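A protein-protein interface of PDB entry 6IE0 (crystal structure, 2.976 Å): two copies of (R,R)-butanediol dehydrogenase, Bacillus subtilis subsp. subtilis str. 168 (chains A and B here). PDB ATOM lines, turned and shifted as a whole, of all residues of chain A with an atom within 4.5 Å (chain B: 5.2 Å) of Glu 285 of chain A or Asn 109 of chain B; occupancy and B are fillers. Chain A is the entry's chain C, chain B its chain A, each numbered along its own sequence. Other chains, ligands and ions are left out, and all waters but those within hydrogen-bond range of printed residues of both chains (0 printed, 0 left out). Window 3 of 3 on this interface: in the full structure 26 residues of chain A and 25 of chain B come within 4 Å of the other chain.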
ATOM      1  N   ALA A 261       6.845 -22.781 -20.951  1.00  0.00           N
ATOM      2  CA  ALA A 261       7.135 -21.368 -20.719  1.00  0.00           C
ATOM      3  C   ALA A 261       8.259 -21.151 -19.714  1.00  0.00           C
ATOM      4  O   ALA A 261       8.381 -20.057 -19.156  1.00  0.00           O
ATOM      5  CB  ALA A 261       5.884 -20.601 -20.274  1.00  0.00           C
ATOM      6  N   ILE A 281      13.748 -24.274 -27.672  1.00  0.00           N
ATOM      7  CA  ILE A 281      13.138 -23.029 -27.223  1.00  0.00           C
ATOM      8  C   ILE A 281      11.746 -22.867 -27.822  1.00  0.00           C
ATOM      9  O   ILE A 281      10.823 -22.382 -27.159  1.00  0.00           O
ATOM     10  CB  ILE A 281      14.058 -21.844 -27.568  1.00  0.00           C
ATOM     11  CG1 ILE A 281      15.407 -21.996 -26.861  1.00  0.00           C
ATOM     12  CG2 ILE A 281      13.404 -20.518 -27.192  1.00  0.00           C
ATOM     13  CD1 ILE A 281      16.426 -20.941 -27.243  1.00  0.00           C
ATOM     14  N   VAL A 282      11.569 -23.286 -29.076  1.00  0.00           N
ATOM     15  CA  VAL A 282      10.319 -23.030 -29.783  1.00  0.00           C
ATOM     16  C   VAL A 282       9.211 -23.963 -29.312  1.00  0.00           C
ATOM     17  O   VAL A 282       8.069 -23.536 -29.125  1.00  0.00           O
ATOM     18  CB  VAL A 282      10.549 -23.168 -31.302  1.00  0.00           C
ATOM     19  CG1 VAL A 282       9.244 -22.982 -32.061  1.00  0.00           C
ATOM     20  CG2 VAL A 282      11.592 -22.186 -31.776  1.00  0.00           C
ATOM     21  N   ILE A 283       9.534 -25.242 -29.103  1.00  0.00           N
ATOM     22  CA  ILE A 283       8.503 -26.254 -28.876  1.00  0.00           C
ATOM     23  C   ILE A 283       7.681 -25.931 -27.633  1.00  0.00           C
ATOM     24  O   ILE A 283       6.446 -25.991 -27.654  1.00  0.00           O
ATOM     25  CB  ILE A 283       9.134 -27.656 -28.797  1.00  0.00           C
ATOM     26  CG1 ILE A 283       9.551 -28.123 -30.194  1.00  0.00           C
ATOM     27  CG2 ILE A 283       8.163 -28.650 -28.185  1.00  0.00           C
ATOM     28  CD1 ILE A 283       8.588 -27.719 -31.299  1.00  0.00           C
ATOM     29  N   LYS A 284       8.347 -25.587 -26.532  1.00  0.00           N
ATOM     30  CA  LYS A 284       7.659 -25.355 -25.268  1.00  0.00           C
ATOM     31  C   LYS A 284       7.580 -23.876 -24.900  1.00  0.00           C
ATOM     32  O   LYS A 284       7.318 -23.547 -23.738  1.00  0.00           O
ATOM     33  CB  LYS A 284       8.326 -26.155 -24.149  1.00  0.00           C
ATOM     34  CG  LYS A 284       8.288 -27.664 -24.366  1.00  0.00           C
ATOM     35  CD  LYS A 284       8.243 -28.418 -23.044  1.00  0.00           C
ATOM     36  CE  LYS A 284       8.503 -29.907 -23.243  1.00  0.00           C
ATOM     37  NZ  LYS A 284       8.918 -30.581 -21.976  1.00  0.00           N
ATOM     38  N   GLU A 285       7.792 -22.980 -25.870  1.00  0.00           N
ATOM     39  CA  GLU A 285       7.689 -21.533 -25.658  1.00  0.00           C
ATOM     40  C   GLU A 285       8.587 -21.074 -24.510  1.00  0.00           C
ATOM     41  O   GLU A 285       8.170 -20.333 -23.615  1.00  0.00           O
ATOM     42  CB  GLU A 285       6.235 -21.114 -25.415  1.00  0.00           C
ATOM     43  CG  GLU A 285       5.325 -21.282 -26.623  1.00  0.00           C
ATOM     44  CD  GLU A 285       4.085 -20.409 -26.549  1.00  0.00           C
ATOM     45  OE1 GLU A 285       3.621 -20.125 -25.424  1.00  0.00           O
ATOM     46  OE2 GLU A 285       3.573 -20.010 -27.616  1.00  0.00           O
ATOM     47  N   ARG A 286       9.838 -21.523 -24.543  1.00  0.00           N
ATOM     48  CA  ARG A 286      10.766 -21.252 -23.460  1.00  0.00           C
ATOM     49  C   ARG A 286      11.398 -19.873 -23.630  1.00  0.00           C
ATOM     50  O   ARG A 286      11.157 -19.160 -24.607  1.00  0.00           O
ATOM     51  CB  ARG A 286      11.829 -22.346 -23.387  1.00  0.00           C
ATOM     52  CG  ARG A 286      11.332 -23.631 -22.747  1.00  0.00           C
ATOM     53  CD  ARG A 286      12.241 -24.804 -23.061  1.00  0.00           C
ATOM     54  NE  ARG A 286      11.831 -26.008 -22.342  1.00  0.00           N
ATOM     55  CZ  ARG A 286      11.861 -27.233 -22.858  1.00  0.00           C
ATOM     56  NH1 ARG A 286      12.283 -27.420 -24.100  1.00  0.00           N
ATOM     57  NH2 ARG A 286      11.472 -28.271 -22.132  1.00  0.00           N
ATOM     58  N   THR A 287      12.209 -19.490 -22.649  1.00  0.00           N
ATOM     59  CA  THR A 287      12.871 -18.196 -22.627  1.00  0.00           C
ATOM     60  C   THR A 287      14.290 -18.382 -22.110  1.00  0.00           C
ATOM     61  O   THR A 287      14.513 -19.085 -21.123  1.00  0.00           O
ATOM     62  CB  THR A 287      12.109 -17.190 -21.745  1.00  0.00           C
ATOM     63  OG1 THR A 287      10.860 -16.856 -22.365  1.00  0.00           O
ATOM     64  CG2 THR A 287      12.922 -15.921 -21.525  1.00  0.00           C
ATOM     65  N   ILE B  98      -7.573 -25.862 -34.182  1.00  0.00           N
ATOM     66  CA  ILE B  98      -6.747 -26.453 -33.133  1.00  0.00           C
ATOM     67  C   ILE B  98      -7.581 -27.457 -32.345  1.00  0.00           C
ATOM     68  O   ILE B  98      -8.625 -27.105 -31.779  1.00  0.00           O
ATOM     69  CB  ILE B  98      -6.156 -25.387 -32.203  1.00  0.00           C
ATOM     70  CG1 ILE B  98      -5.211 -24.471 -32.984  1.00  0.00           C
ATOM     71  CG2 ILE B  98      -5.427 -26.050 -31.043  1.00  0.00           C
ATOM     72  CD1 ILE B  98      -4.361 -23.580 -32.106  1.00  0.00           C
ATOM     73  N   ALA B 107      -3.344 -23.037 -22.228  1.00  0.00           N
ATOM     74  CA  ALA B 107      -2.340 -22.958 -23.286  1.00  0.00           C
ATOM     75  C   ALA B 107      -2.530 -24.123 -24.254  1.00  0.00           C
ATOM     76  O   ALA B 107      -1.703 -25.031 -24.364  1.00  0.00           O
ATOM     77  CB  ALA B 107      -0.938 -22.951 -22.683  1.00  0.00           C
ATOM     78  N   TYR B 108      -3.656 -24.074 -24.974  1.00  0.00           N
ATOM     79  CA  TYR B 108      -4.039 -25.201 -25.816  1.00  0.00           C
ATOM     80  C   TYR B 108      -3.088 -25.408 -26.987  1.00  0.00           C
ATOM     81  O   TYR B 108      -3.016 -26.523 -27.517  1.00  0.00           O
ATOM     82  CB  TYR B 108      -5.479 -25.043 -26.318  1.00  0.00           C
ATOM     83  CG  TYR B 108      -5.846 -23.709 -26.937  1.00  0.00           C
ATOM     84  CD1 TYR B 108      -6.192 -22.623 -26.143  1.00  0.00           C
ATOM     85  CD2 TYR B 108      -5.897 -23.552 -28.317  1.00  0.00           C
ATOM     86  CE1 TYR B 108      -6.552 -21.408 -26.705  1.00  0.00           C
ATOM     87  CE2 TYR B 108      -6.256 -22.341 -28.889  1.00  0.00           C
ATOM     88  CZ  TYR B 108      -6.583 -21.274 -28.076  1.00  0.00           C
ATOM     89  OH  TYR B 108      -6.938 -20.069 -28.634  1.00  0.00           O
ATOM     90  N   ASN B 109      -2.347 -24.377 -27.398  1.00  0.00           N
ATOM     91  CA  ASN B 109      -1.359 -24.574 -28.450  1.00  0.00           C
ATOM     92  C   ASN B 109      -0.171 -25.391 -27.965  1.00  0.00           C
ATOM     93  O   ASN B 109       0.597 -25.896 -28.790  1.00  0.00           O
ATOM     94  CB  ASN B 109      -0.881 -23.225 -28.994  1.00  0.00           C
ATOM     95  CG  ASN B 109      -0.389 -22.295 -27.904  1.00  0.00           C
ATOM     96  OD1 ASN B 109      -0.926 -22.275 -26.795  1.00  0.00           O
ATOM     97  ND2 ASN B 109       0.641 -21.515 -28.214  1.00  0.00           N
ATOM     98  N   LEU B 110      -0.012 -25.539 -26.650  1.00  0.00           N
ATOM     99  CA  LEU B 110       1.061 -26.330 -26.064  1.00  0.00           C
ATOM    100  C   LEU B 110       0.553 -27.617 -25.427  1.00  0.00           C
ATOM    101  O   LEU B 110       1.316 -28.295 -24.730  1.00  0.00           O
ATOM    102  CB  LEU B 110       1.830 -25.498 -25.036  1.00  0.00           C
ATOM    103  CG  LEU B 110       2.431 -24.200 -25.577  1.00  0.00           C
ATOM    104  CD1 LEU B 110       2.923 -23.301 -24.452  1.00  0.00           C
ATOM    105  CD2 LEU B 110       3.555 -24.511 -26.551  1.00  0.00           C
ATOM    106  N   ASP B 111      -0.714 -27.967 -25.646  1.00  0.00           N
ATOM    107  CA  ASP B 111      -1.256 -29.205 -25.104  1.00  0.00           C
ATOM    108  C   ASP B 111      -0.499 -30.408 -25.656  1.00  0.00           C
ATOM    109  O   ASP B 111      -0.077 -30.419 -26.817  1.00  0.00           O
ATOM    110  CB  ASP B 111      -2.746 -29.315 -25.433  1.00  0.00           C
ATOM    111  CG  ASP B 111      -3.417 -30.479 -24.732  1.00  0.00           C
ATOM    112  OD1 ASP B 111      -3.582 -30.415 -23.494  1.00  0.00           O
ATOM    113  OD2 ASP B 111      -3.777 -31.458 -25.419  1.00  0.00           O
ATOM    114  N   MET B 114      -2.085 -32.028 -28.710  1.00  0.00           N
ATOM    115  CA  MET B 114      -2.552 -31.018 -29.651  1.00  0.00           C
ATOM    116  C   MET B 114      -2.463 -31.511 -31.095  1.00  0.00           C
ATOM    117  O   MET B 114      -1.560 -32.267 -31.469  1.00  0.00           O
ATOM    118  CB  MET B 114      -1.738 -29.737 -29.483  1.00  0.00           C
ATOM    119  CG  MET B 114      -2.226 -28.550 -30.293  1.00  0.00           C
ATOM    120  SD  MET B 114      -1.291 -28.329 -31.821  1.00  0.00           S
ATOM    121  CE  MET B 114      -1.337 -26.544 -31.974  1.00  0.00           C
ATOM    122  N   TYR B 160       0.209 -13.375 -33.141  1.00  0.00           N
ATOM    123  CA  TYR B 160       0.531 -13.966 -31.847  1.00  0.00           C
ATOM    124  C   TYR B 160       2.015 -13.841 -31.539  1.00  0.00           C
ATOM    125  O   TYR B 160       2.396 -13.704 -30.371  1.00  0.00           O
ATOM    126  CB  TYR B 160       0.090 -15.428 -31.817  1.00  0.00           C
ATOM    127  CG  TYR B 160       0.481 -16.181 -30.565  1.00  0.00           C
ATOM    128  CD1 TYR B 160      -0.236 -16.027 -29.387  1.00  0.00           C
ATOM    129  CD2 TYR B 160       1.560 -17.057 -30.565  1.00  0.00           C
ATOM    130  CE1 TYR B 160       0.114 -16.718 -28.242  1.00  0.00           C
ATOM    131  CE2 TYR B 160       1.917 -17.754 -29.427  1.00  0.00           C
ATOM    132  CZ  TYR B 160       1.192 -17.579 -28.268  1.00  0.00           C
ATOM    133  OH  TYR B 160       1.546 -18.267 -27.129  1.00  0.00           O
ATOM    134  N   GLY B 290      10.806 -18.287 -27.418  1.00  0.00           N
ATOM    135  CA  GLY B 290      10.247 -19.232 -28.368  1.00  0.00           C
ATOM    136  C   GLY B 290       8.758 -18.999 -28.564  1.00  0.00           C
ATOM    137  O   GLY B 290       8.037 -18.666 -27.626  1.00  0.00           O
ATOM    138  N   ILE B 291       8.309 -19.185 -29.804  1.00  0.00           N
ATOM    139  CA  ILE B 291       6.914 -18.979 -30.177  1.00  0.00           C
ATOM    140  C   ILE B 291       6.489 -20.104 -31.109  1.00  0.00           C
ATOM    141  O   ILE B 291       7.143 -20.353 -32.127  1.00  0.00           O
ATOM    142  CB  ILE B 291       6.707 -17.612 -30.859  1.00  0.00           C
ATOM    143  CG1 ILE B 291       6.679 -16.494 -29.815  1.00  0.00           C
ATOM    144  CG2 ILE B 291       5.433 -17.608 -31.686  1.00  0.00           C
ATOM    145  CD1 ILE B 291       5.651 -16.713 -28.731  1.00  0.00           C
ATOM    146  N   ILE B 292       5.388 -20.772 -30.775  1.00  0.00           N
ATOM    147  CA  ILE B 292       4.831 -21.816 -31.627  1.00  0.00           C
ATOM    148  C   ILE B 292       3.312 -21.714 -31.600  1.00  0.00           C
ATOM    149  O   ILE B 292       2.714 -21.405 -30.563  1.00  0.00           O
ATOM    150  CB  ILE B 292       5.309 -23.224 -31.209  1.00  0.00           C
ATOM    151  CG1 ILE B 292       5.049 -24.226 -32.336  1.00  0.00           C
ATOM    152  CG2 ILE B 292       4.654 -23.672 -29.900  1.00  0.00           C
ATOM    153  CD1 ILE B 292       5.598 -25.607 -32.064  1.00  0.00           C
ATOM    154  N   GLY B 293       2.694 -21.947 -32.754  1.00  0.00           N
ATOM    155  CA  GLY B 293       1.249 -21.866 -32.850  1.00  0.00           C
ATOM    156  C   GLY B 293       0.732 -20.491 -32.479  1.00  0.00           C
ATOM    157  O   GLY B 293       1.333 -19.459 -32.802  1.00  0.00           O
ATOM    158  N   TYR B 294      -0.390 -20.482 -31.767  1.00  0.00           N
ATOM    159  CA  TYR B 294      -1.085 -19.266 -31.361  1.00  0.00           C
ATOM    160  C   TYR B 294      -2.227 -19.684 -30.450  1.00  0.00           C
ATOM    161  O   TYR B 294      -2.613 -20.854 -30.415  1.00  0.00           O
ATOM    162  CB  TYR B 294      -1.619 -18.482 -32.567  1.00  0.00           C
ATOM    163  CG  TYR B 294      -2.449 -19.334 -33.492  1.00  0.00           C
ATOM    164  CD1 TYR B 294      -3.792 -19.576 -33.228  1.00  0.00           C
ATOM    165  CD2 TYR B 294      -1.887 -19.918 -34.614  1.00  0.00           C
ATOM    166  CE1 TYR B 294      -4.550 -20.369 -34.062  1.00  0.00           C
ATOM    167  CE2 TYR B 294      -2.637 -20.709 -35.456  1.00  0.00           C
ATOM    168  CZ  TYR B 294      -3.968 -20.932 -35.175  1.00  0.00           C
ATOM    169  OH  TYR B 294      -4.720 -21.722 -36.006  1.00  0.00           O
ATOM    170  N   ARG B 295      -2.773 -18.710 -29.726  1.00  0.00           N
ATOM    171  CA  ARG B 295      -3.909 -18.970 -28.854  1.00  0.00           C
ATOM    172  C   ARG B 295      -4.573 -17.649 -28.499  1.00  0.00           C
ATOM    173  O   ARG B 295      -3.905 -16.617 -28.376  1.00  0.00           O
ATOM    174  CB  ARG B 295      -3.485 -19.733 -27.591  1.00  0.00           C
ATOM    175  CG  ARG B 295      -2.977 -18.871 -26.446  1.00  0.00           C
ATOM    176  CD  ARG B 295      -2.711 -19.715 -25.213  1.00  0.00           C
ATOM    177  NE  ARG B 295      -1.300 -20.072 -25.093  1.00  0.00           N
ATOM    178  CZ  ARG B 295      -0.399 -19.338 -24.449  1.00  0.00           C
ATOM    179  NH1 ARG B 295      -0.763 -18.201 -23.871  1.00  0.00           N
ATOM    180  NH2 ARG B 295       0.864 -19.733 -24.388  1.00  0.00           N
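Of the printed residues of chain B, Ile 281 of chain A touches Gly 290 (3.4 Å).
Of the printed residues of chain B, Val 282 of chain A touches Ile 291 and Ile 292.
Glu 285 of chain A touches just these residues of chain B: Asn 109, Leu 110, Tyr 160, Gly 290, Ile 292 and Arg 295.
Of the printed residues of chain A, Asn 109 of chain B touches Glu 285.
Of the printed residues of chain A, Gly 290 of chain B touches Ile 281, Glu 285 and Arg 286.
Printed residues of chain A within 4 Å of Ile 291 of chain B: Val 282 (3.4 Å).
Tyr 294 of chain B touches none of the printed residues of chain A.
The nearest residue of chain B that does not touch Glu 285 of chain A is Ile 291 of chain B (4.1 Å).
The nearest printed residue of chain A that does not touch Asn 109 of chain B is Ile 283 of chain A (6.0 Å).
ND2 of Asn 109 of chain B is in hydrogen-bond range of OE2 of Glu 285 of chain A (3.3 Å).
OE2 of Glu 285 of chain A lies within hydrogen-bond range of OH of Tyr 160 of chain B (2.7 Å).
N of Gly 290 of chain B is in hydrogen-bond range of O of Arg 286 of chain A (3.0 Å).
The guanidinium group (NH2) of Arg 295 of chain B lies within salt-bridge range of the side-chain carboxylate (OE1) of Glu 285 of chain A, 3.0 Å away.
OE2 of Glu 285 of chain A sits close to O of Ile 292 of chain B (3.4 Å).
ND2 of Asn 109 of chain B is in hydrogen-bond range of O of Ile 292 of chain B (3.1 Å).
The side-chain amide oxygen (OD1) of Asn 109 of chain B sits at hydrogen-bond distance from the guanidinium group (NE) of Arg 295 of chain B.
The guanidinium group (NH2) of Arg 295 of chain B sits at hydrogen-bond distance from the side-chain hydroxyl (OH) of Tyr 160 of chain B.
O of Ile 281 of chain A lies within hydrogen-bond range of N of Arg 286 of chain A, at 2.9 Å.
Gly 290 of chain B touches Ile 281 of chain A (CA to O, 3.4 Å).
Val 282 of chain A touches Ile 291 of chain B.
Val 282 of chain A touches Ile 292 of chain B (O to CB, 3.5 Å).
Leu 110 of chain B touches Ile 283 of chain A (CD2 to O, 3.4 Å).
Ile 292 of chain B touches Ile 283 of chain A (CG2 to O, 3.7 Å).
Glu 285 of chain A touches Leu 110 of chain B (OE1 to CD1, 3.4 Å).
Gly 290 of chain B touches Glu 285 of chain A.
Of the 8 printed residues of chain A, 5 touch a printed residue of chain B.
Hydrophobic or aromatic side chains of chain A that line the printed part of chain B: Ile 281, Val 282 and Ile 283.
Of the 14 printed residues of chain B, 7 touch a printed residue of chain A.
Printed residues of chain B that touch a printed residue of chain A: Asn 109, Leu 110, Tyr 160, Gly 290, Ile 291, Ile 292 and Arg 295.
Among the printed residues, 12 pairs touch across the chains.
No position is printed for both chains.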
